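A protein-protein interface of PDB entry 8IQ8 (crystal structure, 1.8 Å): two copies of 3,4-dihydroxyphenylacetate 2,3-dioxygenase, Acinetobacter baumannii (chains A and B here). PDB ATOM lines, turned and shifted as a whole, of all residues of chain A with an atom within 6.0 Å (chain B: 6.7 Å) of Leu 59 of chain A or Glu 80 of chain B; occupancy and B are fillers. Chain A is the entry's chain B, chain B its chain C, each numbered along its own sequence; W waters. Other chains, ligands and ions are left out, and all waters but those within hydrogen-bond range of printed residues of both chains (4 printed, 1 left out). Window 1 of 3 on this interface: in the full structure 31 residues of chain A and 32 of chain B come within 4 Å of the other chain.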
ATOM      1  N   ASP A  55       1.495  -8.307  -0.781  1.00  0.00           N
ATOM      2  CA  ASP A  55       2.960  -8.522  -0.699  1.00  0.00           C
ATOM      3  C   ASP A  55       3.668  -7.311  -1.299  1.00  0.00           C
ATOM      4  O   ASP A  55       3.777  -7.215  -2.546  1.00  0.00           O
ATOM      5  CB  ASP A  55       3.366  -9.839  -1.367  1.00  0.00           C
ATOM      6  CG  ASP A  55       4.828 -10.205  -1.160  1.00  0.00           C
ATOM      7  OD1 ASP A  55       5.607  -9.276  -0.932  1.00  0.00           O
ATOM      8  OD2 ASP A  55       5.161 -11.428  -1.187  1.00  0.00           O
ATOM      9  N   SER A  56       4.163  -6.428  -0.427  1.00  0.00           N
ATOM     10  CA  SER A  56       4.814  -5.157  -0.827  1.00  0.00           C
ATOM     11  C   SER A  56       6.253  -5.424  -1.298  1.00  0.00           C
ATOM     12  O   SER A  56       6.948  -4.463  -1.665  1.00  0.00           O
ATOM     13  CB  SER A  56       4.702  -4.128   0.284  1.00  0.00           C
ATOM     14  OG  SER A  56       5.631  -4.360   1.347  1.00  0.00           O
ATOM     15  N   HIS A  57       6.678  -6.690  -1.361  1.00  0.00           N
ATOM     16  CA  HIS A  57       7.958  -7.099  -1.988  1.00  0.00           C
ATOM     17  C   HIS A  57       7.752  -7.551  -3.437  1.00  0.00           C
ATOM     18  O   HIS A  57       8.775  -7.674  -4.142  1.00  0.00           O
ATOM     19  CB  HIS A  57       8.666  -8.163  -1.141  1.00  0.00           C
ATOM     20  CG  HIS A  57      10.148  -8.117  -1.274  1.00  0.00           C
ATOM     21  ND1 HIS A  57      10.832  -8.949  -2.165  1.00  0.00           N
ATOM     22  CD2 HIS A  57      11.080  -7.362  -0.640  1.00  0.00           C
ATOM     23  CE1 HIS A  57      12.132  -8.687  -2.087  1.00  0.00           C
ATOM     24  NE2 HIS A  57      12.303  -7.698  -1.151  1.00  0.00           N
ATOM     25  N   TRP A  58       6.510  -7.738  -3.909  1.00  0.00           N
ATOM     26  CA  TRP A  58       6.237  -8.190  -5.303  1.00  0.00           C
ATOM     27  C   TRP A  58       6.008  -6.979  -6.214  1.00  0.00           C
ATOM     28  O   TRP A  58       4.890  -6.423  -6.199  1.00  0.00           O
ATOM     29  CB  TRP A  58       5.058  -9.169  -5.314  1.00  0.00           C
ATOM     30  CG  TRP A  58       4.623  -9.697  -6.644  1.00  0.00           C
ATOM     31  CD1 TRP A  58       5.227  -9.524  -7.859  1.00  0.00           C
ATOM     32  CD2 TRP A  58       3.516 -10.578  -6.873  1.00  0.00           C
ATOM     33  NE1 TRP A  58       4.546 -10.218  -8.825  1.00  0.00           N
ATOM     34  CE2 TRP A  58       3.479 -10.855  -8.252  1.00  0.00           C
ATOM     35  CE3 TRP A  58       2.525 -11.140  -6.052  1.00  0.00           C
ATOM     36  CZ2 TRP A  58       2.502 -11.676  -8.821  1.00  0.00           C
ATOM     37  CZ3 TRP A  58       1.538 -11.910  -6.623  1.00  0.00           C
ATOM     38  CH2 TRP A  58       1.544 -12.190  -7.983  1.00  0.00           C
ATOM     39  N   LEU A  59       7.004  -6.656  -7.035  1.00  0.00           N
ATOM     40  CA  LEU A  59       7.031  -5.468  -7.930  1.00  0.00           C
ATOM     41  C   LEU A  59       6.287  -5.785  -9.225  1.00  0.00           C
ATOM     42  O   LEU A  59       6.661  -6.774  -9.899  1.00  0.00           O
ATOM     43  CB  LEU A  59       8.473  -5.059  -8.233  1.00  0.00           C
ATOM     44  CG  LEU A  59       8.608  -3.722  -8.974  1.00  0.00           C
ATOM     45  CD1 LEU A  59       9.919  -3.041  -8.610  1.00  0.00           C
ATOM     46  CD2 LEU A  59       8.504  -3.888 -10.489  1.00  0.00           C
ATOM     47  N   VAL A  60       5.279  -4.977  -9.549  1.00  0.00           N
ATOM     48  CA  VAL A  60       4.529  -5.006 -10.835  1.00  0.00           C
ATOM     49  C   VAL A  60       4.428  -3.580 -11.371  1.00  0.00           C
ATOM     50  O   VAL A  60       4.257  -2.648 -10.568  1.00  0.00           O
ATOM     51  CB  VAL A  60       3.140  -5.645 -10.648  1.00  0.00           C
ATOM     52  CG1 VAL A  60       3.270  -7.089 -10.218  1.00  0.00           C
ATOM     53  CG2 VAL A  60       2.295  -4.862  -9.646  1.00  0.00           C
ATOM     54  N   ASN A  61       4.488  -3.422 -12.690  1.00  0.00           N
ATOM     55  CA  ASN A  61       4.365  -2.111 -13.378  1.00  0.00           C
ATOM     56  C   ASN A  61       2.945  -1.921 -13.964  1.00  0.00           C
ATOM     57  O   ASN A  61       2.528  -0.740 -14.185  1.00  0.00           O
ATOM     58  CB  ASN A  61       5.461  -1.987 -14.448  1.00  0.00           C
ATOM     59  CG  ASN A  61       6.875  -1.920 -13.879  1.00  0.00           C
ATOM     60  OD1 ASN A  61       7.190  -1.037 -13.084  1.00  0.00           O
ATOM     61  ND2 ASN A  61       7.754  -2.814 -14.311  1.00  0.00           N
ATOM     62  N   SER A  62       2.242  -3.008 -14.282  1.00  0.00           N
ATOM     63  CA  SER A  62       0.938  -2.988 -15.004  1.00  0.00           C
ATOM     64  C   SER A  62      -0.039  -3.925 -14.301  1.00  0.00           C
ATOM     65  O   SER A  62       0.338  -5.077 -14.107  1.00  0.00           O
ATOM     66  CB  SER A  62       1.132  -3.397 -16.435  1.00  0.00           C
ATOM     67  OG  SER A  62      -0.038  -3.087 -17.187  1.00  0.00           O
ATOM     68  N   HIS A  65      -1.831  -8.236  -9.730  1.00  0.00           N
ATOM     69  CA  HIS A  65      -1.575  -9.659 -10.025  1.00  0.00           C
ATOM     70  C   HIS A  65      -1.834 -10.456  -8.763  1.00  0.00           C
ATOM     71  O   HIS A  65      -1.432 -10.001  -7.684  1.00  0.00           O
ATOM     72  CB  HIS A  65      -0.167  -9.847 -10.570  1.00  0.00           C
ATOM     73  CG  HIS A  65       0.005  -9.210 -11.905  1.00  0.00           C
ATOM     74  ND1 HIS A  65       0.038  -9.954 -13.068  1.00  0.00           N
ATOM     75  CD2 HIS A  65       0.161  -7.916 -12.258  1.00  0.00           C
ATOM     76  CE1 HIS A  65       0.217  -9.135 -14.097  1.00  0.00           C
ATOM     77  NE2 HIS A  65       0.260  -7.868 -13.626  1.00  0.00           N
ATOM     78  N   GLN A 114      -5.336  -9.639 -12.800  1.00  0.00           N
ATOM     79  CA  GLN A 114      -5.065 -10.978 -13.375  1.00  0.00           C
ATOM     80  C   GLN A 114      -4.792 -11.954 -12.234  1.00  0.00           C
ATOM     81  O   GLN A 114      -4.074 -11.549 -11.298  1.00  0.00           O
ATOM     82  CB  GLN A 114      -3.837 -10.941 -14.276  1.00  0.00           C
ATOM     83  CG  GLN A 114      -3.951  -9.934 -15.406  1.00  0.00           C
ATOM     84  CD  GLN A 114      -2.607  -9.762 -16.072  1.00  0.00           C
ATOM     85  OE1 GLN A 114      -1.772 -10.666 -16.052  1.00  0.00           O
ATOM     86  NE2 GLN A 114      -2.377  -8.596 -16.652  1.00  0.00           N
ATOM     87  N   GLU A 124       6.681 -14.513  -3.327  1.00  0.00           N
ATOM     88  CA  GLU A 124       7.663 -13.443  -3.026  1.00  0.00           C
ATOM     89  C   GLU A 124       7.859 -13.322  -1.508  1.00  0.00           C
ATOM     90  O   GLU A 124       7.098 -13.926  -0.722  1.00  0.00           O
ATOM     91  CB  GLU A 124       7.238 -12.134  -3.691  1.00  0.00           C
ATOM     92  CG  GLU A 124       7.986 -11.856  -4.989  1.00  0.00           C
ATOM     93  CD  GLU A 124       9.376 -11.256  -4.835  1.00  0.00           C
ATOM     94  OE1 GLU A 124       9.901 -10.803  -5.854  1.00  0.00           O
ATOM     95  OE2 GLU A 124       9.931 -11.252  -3.702  1.00  0.00           O
ATOM     96  N   SER A 146       0.251  -8.799  -5.599  1.00  0.00           N
ATOM     97  CA  SER A 146       1.320  -7.834  -5.934  1.00  0.00           C
ATOM     98  C   SER A 146       0.951  -6.483  -5.337  1.00  0.00           C
ATOM     99  O   SER A 146      -0.103  -5.929  -5.782  1.00  0.00           O
ATOM    100  CB  SER A 146       1.457  -7.711  -7.429  1.00  0.00           C
ATOM    101  OG  SER A 146       0.270  -7.135  -7.948  1.00  0.00           O
ATOM    102  N   ALA A 147       1.733  -6.014  -4.357  1.00  0.00           N
ATOM    103  CA  ALA A 147       1.517  -4.715  -3.682  1.00  0.00           C
ATOM    104  C   ALA A 147       2.716  -3.760  -3.796  1.00  0.00           C
ATOM    105  O   ALA A 147       2.582  -2.632  -3.235  1.00  0.00           O
ATOM    106  CB  ALA A 147       1.112  -4.914  -2.250  1.00  0.00           C
ATOM    107  N   PHE A 148       3.772  -4.110  -4.526  1.00  0.00           N
ATOM    108  CA  PHE A 148       4.814  -3.151  -5.008  1.00  0.00           C
ATOM    109  C   PHE A 148       4.396  -2.698  -6.412  1.00  0.00           C
ATOM    110  O   PHE A 148       4.846  -3.249  -7.422  1.00  0.00           O
ATOM    111  CB  PHE A 148       6.234  -3.720  -4.882  1.00  0.00           C
ATOM    112  CG  PHE A 148       7.377  -2.743  -5.104  1.00  0.00           C
ATOM    113  CD1 PHE A 148       8.658  -3.061  -4.657  1.00  0.00           C
ATOM    114  CD2 PHE A 148       7.191  -1.492  -5.683  1.00  0.00           C
ATOM    115  CE1 PHE A 148       9.732  -2.205  -4.883  1.00  0.00           C
ATOM    116  CE2 PHE A 148       8.264  -0.622  -5.880  1.00  0.00           C
ATOM    117  CZ  PHE A 148       9.525  -0.971  -5.452  1.00  0.00           C
ATOM    118  N   CYS A 149       3.570  -1.654  -6.444  1.00  0.00           N
ATOM    119  CA  CYS A 149       2.818  -1.182  -7.626  1.00  0.00           C
ATOM    120  C   CYS A 149       3.414   0.164  -8.035  1.00  0.00           C
ATOM    121  O   CYS A 149       3.194   1.156  -7.301  1.00  0.00           O
ATOM    122  CB  CYS A 149       1.328  -1.081  -7.299  1.00  0.00           C
ATOM    123  SG  CYS A 149       0.617  -2.635  -6.690  1.00  0.00           S
ATOM    124  N   THR A 150       4.137   0.203  -9.155  1.00  0.00           N
ATOM    125  CA  THR A 150       4.997   1.365  -9.493  1.00  0.00           C
ATOM    126  C   THR A 150       4.215   2.497 -10.164  1.00  0.00           C
ATOM    127  O   THR A 150       4.720   3.633 -10.171  1.00  0.00           O
ATOM    128  CB  THR A 150       6.155   0.944 -10.399  1.00  0.00           C
ATOM    129  OG1 THR A 150       5.536   0.524 -11.612  1.00  0.00           O
ATOM    130  CG2 THR A 150       7.028  -0.129  -9.774  1.00  0.00           C
ATOM    131  N   PRO B  14      10.720  -6.251 -21.232  1.00  0.00           N
ATOM    132  CA  PRO B  14      10.034  -7.539 -21.414  1.00  0.00           C
ATOM    133  C   PRO B  14       9.387  -7.659 -22.803  1.00  0.00           C
ATOM    134  O   PRO B  14       9.258  -8.779 -23.273  1.00  0.00           O
ATOM    135  CB  PRO B  14       8.980  -7.587 -20.315  1.00  0.00           C
ATOM    136  CG  PRO B  14       9.408  -6.493 -19.345  1.00  0.00           C
ATOM    137  CD  PRO B  14      10.139  -5.443 -20.155  1.00  0.00           C
ATOM    138  N   HIS B  57      17.747  -4.344 -13.111  1.00  0.00           N
ATOM    139  CA  HIS B  57      16.577  -5.120 -12.616  1.00  0.00           C
ATOM    140  C   HIS B  57      16.893  -5.770 -11.260  1.00  0.00           C
ATOM    141  O   HIS B  57      15.934  -6.161 -10.621  1.00  0.00           O
ATOM    142  CB  HIS B  57      16.085  -6.166 -13.645  1.00  0.00           C
ATOM    143  CG  HIS B  57      14.633  -6.503 -13.514  1.00  0.00           C
ATOM    144  ND1 HIS B  57      14.178  -7.567 -12.724  1.00  0.00           N
ATOM    145  CD2 HIS B  57      13.523  -5.923 -14.038  1.00  0.00           C
ATOM    146  CE1 HIS B  57      12.856  -7.635 -12.797  1.00  0.00           C
ATOM    147  NE2 HIS B  57      12.426  -6.620 -13.572  1.00  0.00           N
ATOM    148  N   LEU B  59      17.559  -5.514  -7.556  1.00  0.00           N
ATOM    149  CA  LEU B  59      17.331  -4.498  -6.495  1.00  0.00           C
ATOM    150  C   LEU B  59      18.163  -4.851  -5.252  1.00  0.00           C
ATOM    151  O   LEU B  59      18.041  -5.998  -4.761  1.00  0.00           O
ATOM    152  CB  LEU B  59      15.831  -4.437  -6.164  1.00  0.00           C
ATOM    153  CG  LEU B  59      15.427  -3.315  -5.208  1.00  0.00           C
ATOM    154  CD1 LEU B  59      13.958  -2.964  -5.362  1.00  0.00           C
ATOM    155  CD2 LEU B  59      15.719  -3.686  -3.755  1.00  0.00           C
ATOM    156  N   TYR B  76      13.237 -19.493 -15.951  1.00  0.00           N
ATOM    157  CA  TYR B  76      12.775 -18.155 -15.531  1.00  0.00           C
ATOM    158  C   TYR B  76      11.284 -18.020 -15.871  1.00  0.00           C
ATOM    159  O   TYR B  76      10.850 -18.375 -17.010  1.00  0.00           O
ATOM    160  CB  TYR B  76      13.607 -17.065 -16.204  1.00  0.00           C
ATOM    161  CG  TYR B  76      13.135 -15.676 -15.868  1.00  0.00           C
ATOM    162  CD1 TYR B  76      12.214 -15.020 -16.675  1.00  0.00           C
ATOM    163  CD2 TYR B  76      13.567 -15.045 -14.715  1.00  0.00           C
ATOM    164  CE1 TYR B  76      11.753 -13.751 -16.354  1.00  0.00           C
ATOM    165  CE2 TYR B  76      13.124 -13.773 -14.384  1.00  0.00           C
ATOM    166  CZ  TYR B  76      12.216 -13.125 -15.209  1.00  0.00           C
ATOM    167  OH  TYR B  76      11.794 -11.868 -14.880  1.00  0.00           O
ATOM    168  N   THR B  77      10.536 -17.473 -14.918  1.00  0.00           N
ATOM    169  CA  THR B  77       9.158 -16.977 -15.104  1.00  0.00           C
ATOM    170  C   THR B  77       9.113 -15.552 -14.560  1.00  0.00           C
ATOM    171  O   THR B  77       9.595 -15.336 -13.418  1.00  0.00           O
ATOM    172  CB  THR B  77       8.146 -17.879 -14.386  1.00  0.00           C
ATOM    173  OG1 THR B  77       8.273 -19.185 -14.944  1.00  0.00           O
ATOM    174  CG2 THR B  77       6.728 -17.369 -14.493  1.00  0.00           C
ATOM    175  N   SER B  78       8.604 -14.626 -15.366  1.00  0.00           N
ATOM    176  CA  SER B  78       8.415 -13.214 -14.988  1.00  0.00           C
ATOM    177  C   SER B  78       7.363 -13.137 -13.888  1.00  0.00           C
ATOM    178  O   SER B  78       6.309 -13.819 -13.989  1.00  0.00           O
ATOM    179  CB  SER B  78       8.036 -12.381 -16.159  1.00  0.00           C
ATOM    180  OG  SER B  78       7.753 -11.062 -15.747  1.00  0.00           O
ATOM    181  N   ASN B  79       7.603 -12.295 -12.892  1.00  0.00           N
ATOM    182  CA  ASN B  79       6.547 -11.974 -11.902  1.00  0.00           C
ATOM    183  C   ASN B  79       5.834 -10.673 -12.346  1.00  0.00           C
ATOM    184  O   ASN B  79       4.844 -10.299 -11.695  1.00  0.00           O
ATOM    185  CB  ASN B  79       7.128 -12.002 -10.486  1.00  0.00           C
ATOM    186  CG  ASN B  79       8.031 -10.822 -10.263  1.00  0.00           C
ATOM    187  OD1 ASN B  79       8.269 -10.052 -11.195  1.00  0.00           O
ATOM    188  ND2 ASN B  79       8.557 -10.698  -9.053  1.00  0.00           N
ATOM    189  N   GLU B  80       6.300 -10.024 -13.427  1.00  0.00           N
ATOM    190  CA  GLU B  80       5.651  -8.836 -14.049  1.00  0.00           C
ATOM    191  C   GLU B  80       4.584  -9.327 -15.051  1.00  0.00           C
ATOM    192  O   GLU B  80       3.512  -8.717 -15.074  1.00  0.00           O
ATOM    193  CB  GLU B  80       6.678  -7.906 -14.713  1.00  0.00           C
ATOM    194  CG  GLU B  80       7.411  -6.968 -13.747  1.00  0.00           C
ATOM    195  CD  GLU B  80       8.728  -6.375 -14.248  1.00  0.00           C
ATOM    196  OE1 GLU B  80       8.895  -6.262 -15.491  1.00  0.00           O
ATOM    197  OE2 GLU B  80       9.612  -6.031 -13.394  1.00  0.00           O
ATOM    198  N   LEU B  81       4.876 -10.382 -15.831  1.00  0.00           N
ATOM    199  CA  LEU B  81       4.031 -10.922 -16.935  1.00  0.00           C
ATOM    200  C   LEU B  81       4.079 -12.442 -16.943  1.00  0.00           C
ATOM    201  O   LEU B  81       4.552 -13.048 -17.907  1.00  0.00           O
ATOM    202  CB  LEU B  81       4.569 -10.390 -18.265  1.00  0.00           C
ATOM    203  CG  LEU B  81       4.447  -8.889 -18.466  1.00  0.00           C
ATOM    204  CD1 LEU B  81       5.331  -8.424 -19.610  1.00  0.00           C
ATOM    205  CD2 LEU B  81       2.998  -8.509 -18.716  1.00  0.00           C
ATOM    206  N   PRO B  82       3.581 -13.111 -15.877  1.00  0.00           N
ATOM    207  CA  PRO B  82       3.720 -14.556 -15.746  1.00  0.00           C
ATOM    208  C   PRO B  82       3.114 -15.409 -16.865  1.00  0.00           C
ATOM    209  O   PRO B  82       3.654 -16.446 -17.152  1.00  0.00           O
ATOM    210  CB  PRO B  82       2.991 -14.926 -14.450  1.00  0.00           C
ATOM    211  CG  PRO B  82       2.680 -13.634 -13.761  1.00  0.00           C
ATOM    212  CD  PRO B  82       2.926 -12.492 -14.721  1.00  0.00           C
ATOM    213  N   HIS B  83       1.997 -14.970 -17.452  1.00  0.00           N
ATOM    214  CA  HIS B  83       1.282 -15.710 -18.529  1.00  0.00           C
ATOM    215  C   HIS B  83       2.156 -15.826 -19.785  1.00  0.00           C
ATOM    216  O   HIS B  83       2.103 -16.887 -20.435  1.00  0.00           O
ATOM    217  CB  HIS B  83      -0.071 -15.058 -18.858  1.00  0.00           C
ATOM    218  CG  HIS B  83      -0.769 -15.704 -20.010  1.00  0.00           C
ATOM    219  ND1 HIS B  83      -1.066 -17.058 -20.034  1.00  0.00           N
ATOM    220  CD2 HIS B  83      -1.216 -15.199 -21.183  1.00  0.00           C
ATOM    221  CE1 HIS B  83      -1.661 -17.357 -21.172  1.00  0.00           C
ATOM    222  NE2 HIS B  83      -1.769 -16.233 -21.895  1.00  0.00           N
ATOM    223  N   TYR B 125      16.845 -10.427 -14.440  1.00  0.00           N
ATOM    224  CA  TYR B 125      16.282 -10.235 -15.793  1.00  0.00           C
ATOM    225  C   TYR B 125      17.177  -9.354 -16.657  1.00  0.00           C
ATOM    226  O   TYR B 125      17.278  -9.657 -17.847  1.00  0.00           O
ATOM    227  CB  TYR B 125      14.844  -9.699 -15.697  1.00  0.00           C
ATOM    228  CG  TYR B 125      14.065  -9.934 -16.956  1.00  0.00           C
ATOM    229  CD1 TYR B 125      13.863 -11.218 -17.420  1.00  0.00           C
ATOM    230  CD2 TYR B 125      13.561  -8.879 -17.705  1.00  0.00           C
ATOM    231  CE1 TYR B 125      13.208 -11.460 -18.613  1.00  0.00           C
ATOM    232  CE2 TYR B 125      12.874  -9.110 -18.890  1.00  0.00           C
ATOM    233  CZ  TYR B 125      12.706 -10.406 -19.355  1.00  0.00           C
ATOM    234  OH  TYR B 125      12.019 -10.672 -20.513  1.00  0.00           O
ATOM    235  N   PHE B 148      20.006  -1.830  -9.479  1.00  0.00           N
ATOM    236  CA  PHE B 148      18.784  -1.203  -8.888  1.00  0.00           C
ATOM    237  C   PHE B 148      19.141  -0.913  -7.425  1.00  0.00           C
ATOM    238  O   PHE B 148      18.824  -1.698  -6.530  1.00  0.00           O
ATOM    239  CB  PHE B 148      17.536  -2.068  -9.145  1.00  0.00           C
ATOM    240  CG  PHE B 148      16.194  -1.468  -8.785  1.00  0.00           C
ATOM    241  CD1 PHE B 148      15.028  -1.963  -9.364  1.00  0.00           C
ATOM    242  CD2 PHE B 148      16.079  -0.396  -7.903  1.00  0.00           C
ATOM    243  CE1 PHE B 148      13.788  -1.420  -9.060  1.00  0.00           C
ATOM    244  CE2 PHE B 148      14.840   0.156  -7.612  1.00  0.00           C
ATOM    245  CZ  PHE B 148      13.707  -0.336  -8.205  1.00  0.00           C
ATOM    246  N   PHE B 187       7.189   4.659 -15.978  1.00  0.00           N
ATOM    247  CA  PHE B 187       6.359   3.602 -16.588  1.00  0.00           C
ATOM    248  C   PHE B 187       4.928   4.163 -16.746  1.00  0.00           C
ATOM    249  O   PHE B 187       4.440   4.921 -15.880  1.00  0.00           O
ATOM    250  CB  PHE B 187       6.427   2.330 -15.739  1.00  0.00           C
ATOM    251  CG  PHE B 187       5.978   1.075 -16.445  1.00  0.00           C
ATOM    252  CD1 PHE B 187       6.909   0.177 -16.967  1.00  0.00           C
ATOM    253  CD2 PHE B 187       4.636   0.822 -16.650  1.00  0.00           C
ATOM    254  CE1 PHE B 187       6.489  -0.968 -17.625  1.00  0.00           C
ATOM    255  CE2 PHE B 187       4.221  -0.325 -17.313  1.00  0.00           C
ATOM    256  CZ  PHE B 187       5.141  -1.223 -17.779  1.00  0.00           C
HETATM  257  O   HOH W   1       9.202  -8.558  -7.106  1.00  0.00           O
HETATM  258  O   HOH W   2      10.378  -3.206 -13.556  1.00  0.00           O
HETATM  259  O   HOH W   3       7.149  -4.702 -16.874  1.00  0.00           O
HETATM  260  O   HOH W   4       3.635  -5.669 -14.742  1.00  0.00           O
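O of Asn 79 of chain B sits at hydrogen-bond distance from NE1 of Trp 58 of chain A (2.9 Å). The side-chain carboxylate of Glu 124 of chain A lies within hydrogen-bond range of the side-chain amide nitrogen of Asn 79 of chain B.
The side-chain hydroxyl of Thr 150 of chain A sits at hydrogen-bond distance from the side-chain amide oxygen of Asn 61 of chain A. N of Thr 150 of chain A sits at hydrogen-bond distance from O of Val 60 of chain A, at 3.2 Å. The backbone NH (N) of Phe 148 of chain A sits at hydrogen-bond distance from the backbone carbonyl oxygen (O) of Trp 58 of chain A, at 3.1 Å. O of Phe 148 of chain A is in hydrogen-bond range of N of Val 60 of chain A, at 2.8 Å. The side-chain carboxylate (OE2) of Glu 124 of chain A is in hydrogen-bond range of a ring nitrogen (ND1) of His 57 of chain A, 2.9 Å away. The side-chain carboxylate (OD1) of Asp 55 of chain A lies within hydrogen-bond range of the backbone NH (N) of Trp 58 of chain A (3.5 Å).
Among the printed residues, pairs that only touch across the chains: Leu 59 of chain A with Asn 79 of chain B (3.9 Å), Leu 59 of chain A with Glu 80 of chain B (3.8 Å), Val 60 of chain A with Asn 79 of chain B (3.9 Å), Asn 61 of chain A with Glu 80 of chain B (3.7 Å), Asn 61 of chain A with Phe 187 of chain B (3.4 Å) and His 65 of chain A with Glu 80 of chain B (3.5 Å).
Printed residues of chain B within 4 Å of Asn 61 of chain A: Glu 80 and Phe 187. Ser 62 of chain A touches none of the printed residues of chain B. Of the printed residues of chain B, His 65 of chain A touches Glu 80. Leu 59 of chain B touches none of the printed residues of chain A. Glu 80 of chain B touches just these residues of chain A: Leu 59 (3.8 Å), Asn 61 (3.7 Å) and His 65 (3.5 Å). The nearest residue of chain B that does not touch Leu 59 of chain A is Phe 148 of chain B (4.2 Å). The nearest printed residue of chain B that does not touch His 65 of chain A is Pro 82 of chain B (4.2 Å).
Printed residues of chain A that touch a printed residue of chain B: Trp 58, Leu 59, Val 60, Asn 61, His 65 and Glu 124. Hydrophobic or aromatic side chains of chain A that line the printed part of chain B: Trp 58, Leu 59, Val 60 and His 65. Of the 14 printed residues of chain B, 3 touch a printed residue of chain A. Among the printed residues, 8 pairs touch across the chains.
3 positions are printed for both chains.
Water W1 lies within hydrogen-bond range of the side-chain carboxylate of Glu 124 of chain A (2.7 Å), the backbone NH of Leu 59 of chain A (2.9 Å), the side-chain amide nitrogen of Asn 79 of chain B (3.0 Å) and the backbone carbonyl oxygen of His 57 of chain A (3.1 Å). Water W3 bridges OE1 of Glu 80 of chain B and ND2 of Asn 61 of chain A. Water W2 bridges ND2 of Asn 61 of chain A (2.8 Å) and OE2 of Glu 80 of chain B (2.9 Å). Water W4 lies within hydrogen-bond range of the backbone NH (N) of Ser 62 of chain A (3.0 Å), the backbone carbonyl oxygen (O) of Glu 80 of chain B (3.1 Å) and the backbone NH (N) of Asn 61 of chain A (3.2 Å).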
